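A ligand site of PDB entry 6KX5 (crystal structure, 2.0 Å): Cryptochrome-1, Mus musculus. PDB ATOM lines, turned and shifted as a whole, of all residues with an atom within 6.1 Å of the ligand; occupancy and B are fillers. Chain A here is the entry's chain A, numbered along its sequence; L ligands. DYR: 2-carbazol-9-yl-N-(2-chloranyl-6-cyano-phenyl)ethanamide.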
ATOM      1  N   GLN A 291      15.217  -3.763  11.067  1.00  0.00           N
ATOM      2  CA  GLN A 291      14.801  -3.327   9.732  1.00  0.00           C
ATOM      3  C   GLN A 291      15.175  -4.336   8.646  1.00  0.00           C
ATOM      4  O   GLN A 291      14.333  -4.723   7.821  1.00  0.00           O
ATOM      5  CB  GLN A 291      15.435  -1.964   9.443  1.00  0.00           C
ATOM      6  N   TRP A 294      13.102  -7.659   8.468  1.00  0.00           N
ATOM      7  CA  TRP A 294      11.768  -7.487   7.911  1.00  0.00           C
ATOM      8  C   TRP A 294      11.809  -7.409   6.384  1.00  0.00           C
ATOM      9  O   TRP A 294      10.871  -7.875   5.700  1.00  0.00           O
ATOM     10  CB  TRP A 294      11.108  -6.225   8.503  1.00  0.00           C
ATOM     11  CG  TRP A 294      10.483  -6.430   9.862  1.00  0.00           C
ATOM     12  CD1 TRP A 294      10.896  -5.880  11.042  1.00  0.00           C
ATOM     13  CD2 TRP A 294       9.312  -7.212  10.167  1.00  0.00           C
ATOM     14  NE1 TRP A 294      10.063  -6.296  12.066  1.00  0.00           N
ATOM     15  CE2 TRP A 294       9.089  -7.110  11.556  1.00  0.00           C
ATOM     16  CE3 TRP A 294       8.436  -7.998   9.394  1.00  0.00           C
ATOM     17  CZ2 TRP A 294       8.029  -7.749  12.192  1.00  0.00           C
ATOM     18  CZ3 TRP A 294       7.385  -8.642  10.034  1.00  0.00           C
ATOM     19  CH2 TRP A 294       7.189  -8.517  11.415  1.00  0.00           C
ATOM     20  N   ARG A 295      12.871  -6.825   5.837  1.00  0.00           N
ATOM     21  CA  ARG A 295      13.070  -6.792   4.395  1.00  0.00           C
ATOM     22  C   ARG A 295      13.111  -8.208   3.817  1.00  0.00           C
ATOM     23  O   ARG A 295      12.414  -8.510   2.831  1.00  0.00           O
ATOM     24  CB  ARG A 295      14.376  -6.072   4.097  1.00  0.00           C
ATOM     25  CG  ARG A 295      14.406  -5.332   2.824  1.00  0.00           C
ATOM     26  CD  ARG A 295      15.636  -4.425   2.782  1.00  0.00           C
ATOM     27  NE  ARG A 295      16.094  -4.333   1.408  1.00  0.00           N
ATOM     28  CZ  ARG A 295      16.970  -5.151   0.851  1.00  0.00           C
ATOM     29  NH1 ARG A 295      17.521  -6.138   1.551  1.00  0.00           N
ATOM     30  NH2 ARG A 295      17.308  -4.972  -0.424  1.00  0.00           N
ATOM     31  N   PHE A 298       9.526 -10.163   3.910  1.00  0.00           N
ATOM     32  CA  PHE A 298       8.519  -9.926   2.878  1.00  0.00           C
ATOM     33  C   PHE A 298       8.966 -10.447   1.518  1.00  0.00           C
ATOM     34  O   PHE A 298       8.145 -10.955   0.744  1.00  0.00           O
ATOM     35  CB  PHE A 298       8.191  -8.443   2.846  1.00  0.00           C
ATOM     36  CG  PHE A 298       7.368  -7.981   4.017  1.00  0.00           C
ATOM     37  CD1 PHE A 298       6.111  -8.530   4.253  1.00  0.00           C
ATOM     38  CD2 PHE A 298       7.853  -7.022   4.886  1.00  0.00           C
ATOM     39  CE1 PHE A 298       5.331  -8.091   5.300  1.00  0.00           C
ATOM     40  CE2 PHE A 298       7.093  -6.574   5.954  1.00  0.00           C
ATOM     41  CZ  PHE A 298       5.828  -7.105   6.175  1.00  0.00           C
ATOM     42  N   HIS A 357       7.855   5.618   8.615  1.00  0.00           N
ATOM     43  CA  HIS A 357       7.127   4.344   8.652  1.00  0.00           C
ATOM     44  C   HIS A 357       5.813   4.474   9.397  1.00  0.00           C
ATOM     45  O   HIS A 357       4.797   3.927   8.972  1.00  0.00           O
ATOM     46  CB  HIS A 357       7.979   3.240   9.282  1.00  0.00           C
ATOM     47  CG  HIS A 357       8.882   2.565   8.298  1.00  0.00           C
ATOM     48  ND1 HIS A 357       9.464   1.331   8.555  1.00  0.00           N
ATOM     49  CD2 HIS A 357       9.298   2.923   7.066  1.00  0.00           C
ATOM     50  CE1 HIS A 357      10.202   0.977   7.512  1.00  0.00           C
ATOM     51  NE2 HIS A 357      10.121   1.928   6.601  1.00  0.00           N
ATOM     52  N   LEU A 358       5.797   5.219  10.511  1.00  0.00           N
ATOM     53  CA  LEU A 358       4.564   5.318  11.282  1.00  0.00           C
ATOM     54  C   LEU A 358       3.528   6.201  10.605  1.00  0.00           C
ATOM     55  O   LEU A 358       2.321   6.030  10.807  1.00  0.00           O
ATOM     56  CB  LEU A 358       4.855   5.850  12.680  1.00  0.00           C
ATOM     57  CG  LEU A 358       5.578   4.843  13.572  1.00  0.00           C
ATOM     58  CD1 LEU A 358       5.586   5.380  15.003  1.00  0.00           C
ATOM     59  CD2 LEU A 358       4.922   3.482  13.509  1.00  0.00           C
ATOM     60  N   ARG A 360       3.187   6.097   7.358  1.00  0.00           N
ATOM     61  CA  ARG A 360       2.606   5.143   6.411  1.00  0.00           C
ATOM     62  C   ARG A 360       1.486   4.346   7.070  1.00  0.00           C
ATOM     63  O   ARG A 360       0.434   4.114   6.460  1.00  0.00           O
ATOM     64  CB  ARG A 360       3.691   4.197   5.861  1.00  0.00           C
ATOM     65  CG  ARG A 360       4.882   4.942   5.145  1.00  0.00           C
ATOM     66  CD  ARG A 360       6.065   4.007   4.796  1.00  0.00           C
ATOM     67  NE  ARG A 360       7.315   4.769   4.616  1.00  0.00           N
ATOM     68  CZ  ARG A 360       8.370   4.381   3.888  1.00  0.00           C
ATOM     69  NH1 ARG A 360       9.447   5.167   3.793  1.00  0.00           N
ATOM     70  NH2 ARG A 360       8.352   3.216   3.256  1.00  0.00           N
ATOM     71  N   HIS A 361       1.699   3.895   8.321  1.00  0.00           N
ATOM     72  CA  HIS A 361       0.657   3.209   9.075  1.00  0.00           C
ATOM     73  C   HIS A 361      -0.598   4.059   9.157  1.00  0.00           C
ATOM     74  O   HIS A 361      -1.725   3.555   9.002  1.00  0.00           O
ATOM     75  CB  HIS A 361       1.131   2.892  10.507  1.00  0.00           C
ATOM     76  CG  HIS A 361       2.091   1.750  10.612  1.00  0.00           C
ATOM     77  ND1 HIS A 361       1.861   0.668  11.429  1.00  0.00           N
ATOM     78  CD2 HIS A 361       3.284   1.527  10.018  1.00  0.00           C
ATOM     79  CE1 HIS A 361       2.879  -0.175  11.336  1.00  0.00           C
ATOM     80  NE2 HIS A 361       3.760   0.324  10.491  1.00  0.00           N
ATOM     81  N   ALA A 364      -2.348   4.463   5.734  1.00  0.00           N
ATOM     82  CA  ALA A 364      -2.825   3.166   5.247  1.00  0.00           C
ATOM     83  C   ALA A 364      -4.045   2.697   6.034  1.00  0.00           C
ATOM     84  O   ALA A 364      -4.988   2.139   5.466  1.00  0.00           O
ATOM     85  CB  ALA A 364      -1.723   2.110   5.333  1.00  0.00           C
ATOM     86  N   PHE A 383       1.348   4.177  -3.488  1.00  0.00           N
ATOM     87  CA  PHE A 383       2.660   4.111  -2.862  1.00  0.00           C
ATOM     88  C   PHE A 383       3.716   3.652  -3.867  1.00  0.00           C
ATOM     89  O   PHE A 383       4.831   4.191  -3.883  1.00  0.00           O
ATOM     90  CB  PHE A 383       2.616   3.189  -1.643  1.00  0.00           C
ATOM     91  CG  PHE A 383       2.246   3.868  -0.343  1.00  0.00           C
ATOM     92  CD1 PHE A 383       1.467   5.014  -0.329  1.00  0.00           C
ATOM     93  CD2 PHE A 383       2.664   3.335   0.870  1.00  0.00           C
ATOM     94  CE1 PHE A 383       1.115   5.637   0.890  1.00  0.00           C
ATOM     95  CE2 PHE A 383       2.333   3.949   2.088  1.00  0.00           C
ATOM     96  CZ  PHE A 383       1.563   5.105   2.095  1.00  0.00           C
ATOM     97  N   LEU A 387       6.515   6.447  -3.570  1.00  0.00           N
ATOM     98  CA  LEU A 387       7.436   6.114  -2.492  1.00  0.00           C
ATOM     99  C   LEU A 387       8.746   5.550  -3.049  1.00  0.00           C
ATOM    100  O   LEU A 387       8.736   4.511  -3.708  1.00  0.00           O
ATOM    101  CB  LEU A 387       6.800   5.057  -1.589  1.00  0.00           C
ATOM    102  CG  LEU A 387       6.365   5.336  -0.173  1.00  0.00           C
ATOM    103  CD1 LEU A 387       6.285   4.010   0.588  1.00  0.00           C
ATOM    104  CD2 LEU A 387       7.303   6.321   0.490  1.00  0.00           C
ATOM    105  N   ASP A 389      11.283   4.034  -1.493  1.00  0.00           N
ATOM    106  CA  ASP A 389      11.713   2.753  -0.933  1.00  0.00           C
ATOM    107  C   ASP A 389      10.634   1.662  -1.012  1.00  0.00           C
ATOM    108  O   ASP A 389      10.690   0.691  -0.257  1.00  0.00           O
ATOM    109  CB  ASP A 389      12.181   2.923   0.529  1.00  0.00           C
ATOM    110  CG  ASP A 389      11.105   3.419   1.460  1.00  0.00           C
ATOM    111  OD1 ASP A 389       9.916   3.397   1.077  1.00  0.00           O
ATOM    112  OD2 ASP A 389      11.450   3.840   2.605  1.00  0.00           O
ATOM    113  N   ALA A 390       9.691   1.799  -1.928  1.00  0.00           N
ATOM    114  CA  ALA A 390       8.553   0.886  -1.987  1.00  0.00           C
ATOM    115  C   ALA A 390       8.804  -0.202  -3.033  1.00  0.00           C
ATOM    116  O   ALA A 390       8.192  -0.233  -4.095  1.00  0.00           O
ATOM    117  CB  ALA A 390       7.273   1.644  -2.284  1.00  0.00           C
ATOM    118  N   ASP A 391       9.708  -1.111  -2.716  1.00  0.00           N
ATOM    119  CA  ASP A 391       9.769  -2.248  -3.620  1.00  0.00           C
ATOM    120  C   ASP A 391       8.564  -3.145  -3.379  1.00  0.00           C
ATOM    121  O   ASP A 391       7.923  -3.117  -2.320  1.00  0.00           O
ATOM    122  CB  ASP A 391      11.084  -3.021  -3.472  1.00  0.00           C
ATOM    123  CG  ASP A 391      11.351  -3.487  -2.064  1.00  0.00           C
ATOM    124  OD1 ASP A 391      10.565  -4.318  -1.558  1.00  0.00           O
ATOM    125  OD2 ASP A 391      12.352  -3.028  -1.472  1.00  0.00           O
ATOM    126  N   ILE A 394       7.810  -5.601  -0.164  1.00  0.00           N
ATOM    127  CA  ILE A 394       7.575  -4.947   1.133  1.00  0.00           C
ATOM    128  C   ILE A 394       6.331  -4.072   1.087  1.00  0.00           C
ATOM    129  O   ILE A 394       5.592  -3.986   2.079  1.00  0.00           O
ATOM    130  CB  ILE A 394       8.809  -4.129   1.566  1.00  0.00           C
ATOM    131  CG1 ILE A 394      10.083  -4.983   1.516  1.00  0.00           C
ATOM    132  CG2 ILE A 394       8.588  -3.531   2.980  1.00  0.00           C
ATOM    133  CD1 ILE A 394      11.387  -4.165   1.474  1.00  0.00           C
ATOM    134  N   ASN A 395       6.053  -3.450  -0.057  1.00  0.00           N
ATOM    135  CA  ASN A 395       4.896  -2.573  -0.184  1.00  0.00           C
ATOM    136  C   ASN A 395       3.595  -3.374  -0.128  1.00  0.00           C
ATOM    137  O   ASN A 395       2.683  -3.048   0.644  1.00  0.00           O
ATOM    138  CB  ASN A 395       5.003  -1.761  -1.485  1.00  0.00           C
ATOM    139  CG  ASN A 395       3.929  -0.664  -1.611  1.00  0.00           C
ATOM    140  OD1 ASN A 395       3.525  -0.042  -0.627  1.00  0.00           O
ATOM    141  ND2 ASN A 395       3.502  -0.413  -2.846  1.00  0.00           N
ATOM    142  N   ALA A 396       3.486  -4.434  -0.945  1.00  0.00           N
ATOM    143  CA  ALA A 396       2.297  -5.282  -0.894  1.00  0.00           C
ATOM    144  C   ALA A 396       2.162  -5.962   0.465  1.00  0.00           C
ATOM    145  O   ALA A 396       1.066  -6.032   1.030  1.00  0.00           O
ATOM    146  CB  ALA A 396       2.361  -6.326  -2.015  1.00  0.00           C
ATOM    147  N   GLY A 397       3.271  -6.467   1.008  1.00  0.00           N
ATOM    148  CA  GLY A 397       3.235  -7.059   2.337  1.00  0.00           C
ATOM    149  C   GLY A 397       2.732  -6.100   3.404  1.00  0.00           C
ATOM    150  O   GLY A 397       1.870  -6.454   4.218  1.00  0.00           O
ATOM    151  N   SER A 398       3.263  -4.874   3.417  1.00  0.00           N
ATOM    152  CA  SER A 398       2.875  -3.913   4.450  1.00  0.00           C
ATOM    153  C   SER A 398       1.399  -3.536   4.340  1.00  0.00           C
ATOM    154  O   SER A 398       0.724  -3.328   5.364  1.00  0.00           O
ATOM    155  CB  SER A 398       3.750  -2.641   4.383  1.00  0.00           C
ATOM    156  OG  SER A 398       5.115  -2.916   4.698  1.00  0.00           O
ATOM    157  N   TRP A 399       0.891  -3.384   3.109  1.00  0.00           N
ATOM    158  CA  TRP A 399      -0.506  -2.978   2.915  1.00  0.00           C
ATOM    159  C   TRP A 399      -1.463  -4.086   3.356  1.00  0.00           C
ATOM    160  O   TRP A 399      -2.542  -3.803   3.905  1.00  0.00           O
ATOM    161  CB  TRP A 399      -0.730  -2.595   1.447  1.00  0.00           C
ATOM    162  CG  TRP A 399      -0.416  -1.151   1.175  1.00  0.00           C
ATOM    163  CD1 TRP A 399       0.722  -0.656   0.627  1.00  0.00           C
ATOM    164  CD2 TRP A 399      -1.236  -0.019   1.478  1.00  0.00           C
ATOM    165  NE1 TRP A 399       0.653   0.714   0.538  1.00  0.00           N
ATOM    166  CE2 TRP A 399      -0.537   1.140   1.071  1.00  0.00           C
ATOM    167  CE3 TRP A 399      -2.503   0.137   2.069  1.00  0.00           C
ATOM    168  CZ2 TRP A 399      -1.046   2.425   1.226  1.00  0.00           C
ATOM    169  CZ3 TRP A 399      -3.024   1.431   2.207  1.00  0.00           C
ATOM    170  CH2 TRP A 399      -2.295   2.559   1.780  1.00  0.00           C
ATOM    171  N   TRP A 401      -0.637  -6.216   5.763  1.00  0.00           N
ATOM    172  CA  TRP A 401      -0.494  -6.170   7.224  1.00  0.00           C
ATOM    173  C   TRP A 401      -1.373  -5.094   7.830  1.00  0.00           C
ATOM    174  O   TRP A 401      -2.132  -5.356   8.771  1.00  0.00           O
ATOM    175  CB  TRP A 401       0.975  -5.943   7.589  1.00  0.00           C
ATOM    176  CG  TRP A 401       1.319  -5.967   9.065  1.00  0.00           C
ATOM    177  CD1 TRP A 401       0.969  -5.049  10.016  1.00  0.00           C
ATOM    178  CD2 TRP A 401       2.136  -6.951   9.726  1.00  0.00           C
ATOM    179  NE1 TRP A 401       1.496  -5.420  11.239  1.00  0.00           N
ATOM    180  CE2 TRP A 401       2.216  -6.573  11.077  1.00  0.00           C
ATOM    181  CE3 TRP A 401       2.792  -8.104   9.300  1.00  0.00           C
ATOM    182  CZ2 TRP A 401       2.936  -7.321  12.017  1.00  0.00           C
ATOM    183  CZ3 TRP A 401       3.508  -8.835  10.217  1.00  0.00           C
ATOM    184  CH2 TRP A 401       3.572  -8.447  11.561  1.00  0.00           C
ATOM    185  N   LEU A 402      -1.305  -3.871   7.293  1.00  0.00           N
ATOM    186  CA  LEU A 402      -2.012  -2.730   7.871  1.00  0.00           C
ATOM    187  C   LEU A 402      -3.528  -2.881   7.752  1.00  0.00           C
ATOM    188  O   LEU A 402      -4.259  -2.489   8.665  1.00  0.00           O
ATOM    189  CB  LEU A 402      -1.578  -1.434   7.187  1.00  0.00           C
ATOM    190  CG  LEU A 402      -0.548  -0.620   7.978  1.00  0.00           C
ATOM    191  CD1 LEU A 402      -1.064  -0.172   9.348  1.00  0.00           C
ATOM    192  CD2 LEU A 402       0.670  -1.452   8.134  1.00  0.00           C
HETATM  193  C10 DYR L   1       3.067   0.492   3.161  1.00  0.00           C
HETATM  194  C13 DYR L   1       3.272   0.765   5.939  1.00  0.00           C
HETATM  195  C15 DYR L   1       6.251  -0.609   7.773  1.00  0.00           C
HETATM  196  C20 DYR L   1       7.127  -4.837   9.249  1.00  0.00           C
HETATM  197  C21 DYR L   1       5.923  -5.326   9.710  1.00  0.00           C
HETATM  198  C22 DYR L   1       4.752  -4.700   9.339  1.00  0.00           C
HETATM  199  C01 DYR L   1       7.610  -0.061   1.836  1.00  0.00           C
HETATM  200  C02 DYR L   1       6.221   0.079   2.004  1.00  0.00           C
HETATM  201  C03 DYR L   1       5.684   0.265   3.292  1.00  0.00           C
HETATM  202  C04 DYR L   1       6.512   0.301   4.401  1.00  0.00           C
HETATM  203  C05 DYR L   1       7.917   0.166   4.230  1.00  0.00           C
HETATM  204  C06 DYR L   1       8.437  -0.016   2.956  1.00  0.00           C
HETATM  205  C08 DYR L   1       4.445   0.594   5.160  1.00  0.00           C
HETATM  206  C09 DYR L   1       4.329   0.457   3.798  1.00  0.00           C
HETATM  207  C11 DYR L   1       1.915   0.677   3.938  1.00  0.00           C
HETATM  208  C12 DYR L   1       2.034   0.818   5.324  1.00  0.00           C
HETATM  209  C14 DYR L   1       6.252   0.633   6.895  1.00  0.00           C
HETATM  210  C18 DYR L   1       6.015  -3.085   8.058  1.00  0.00           C
HETATM  211  C19 DYR L   1       7.182  -3.712   8.438  1.00  0.00           C
HETATM  212  C23 DYR L   1       4.811  -3.584   8.508  1.00  0.00           C
HETATM  213  C25 DYR L   1       8.510  -3.189   7.936  1.00  0.00           C
HETATM  214  N07 DYR L   1       5.749   0.493   5.517  1.00  0.00           N
HETATM  215  N17 DYR L   1       6.025  -1.915   7.183  1.00  0.00           N
HETATM  216  N26 DYR L   1       9.489  -2.774   7.555  1.00  0.00           N
HETATM  217  O16 DYR L   1       6.436  -0.503   8.945  1.00  0.00           O
HETATM  218 CL1  DYR L   1       3.322  -2.762   8.047  1.00  0.00          CL
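OG of Ser 398 sits at hydrogen-bond distance from O of Ile 394 (2.9 Å). NH1 of Arg 360 lies within salt-bridge range of OD2 of Asp 389, 2.7 Å away. The backbone NH of Ile 394 lies close to the side-chain carboxylate of Asp 391 (3.3 Å). NE1 of Trp 399 lies close to OD1 of Asn 395, at 3.2 Å.
N17 of the ligand sits at hydrogen-bond distance from OG of Ser 398 (2.8 Å). NE2 of His 361 lies within hydrogen-bond range of O16 of the ligand (3.2 Å).
CD2 of Trp 294 touches C20 of the ligand, 3.4 Å away. Phe 298 touches the ligand (CE2 to C20, 3.7 Å). His 357 touches the ligand (CG to C14, 3.6 Å). Arg 360 touches the ligand (NH2 to C05, 3.2 Å). Ala 364 touches the ligand (CB to C12, 3.97 Å). CD2 of Phe 383 touches C10 of the ligand (3.7 Å). Asp 389 touches the ligand (O to C01, 3.8 Å). Ile 394 touches the ligand (CG2 to C06, 3.5 Å). Asn 395 touches the ligand (CA to C02, 3.7 Å). Trp 399 touches the ligand (NE1 to C10, 3.6 Å). Trp 401 touches the ligand. Leu 402 touches the ligand (CD2 to CL1, 3.0 Å). Hydrophobic or aromatic side chains within 4 Å of the ligand: Trp 294, Phe 298, His 357, His 361, Ala 364, Phe 383, Ile 394, Trp 399, Trp 401 and Leu 402. Of the 22 residues printed, 14 come within 4 Å of the ligand. The nearest printed residue that does not touch the ligand is Ala 390 (4.05 Å).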
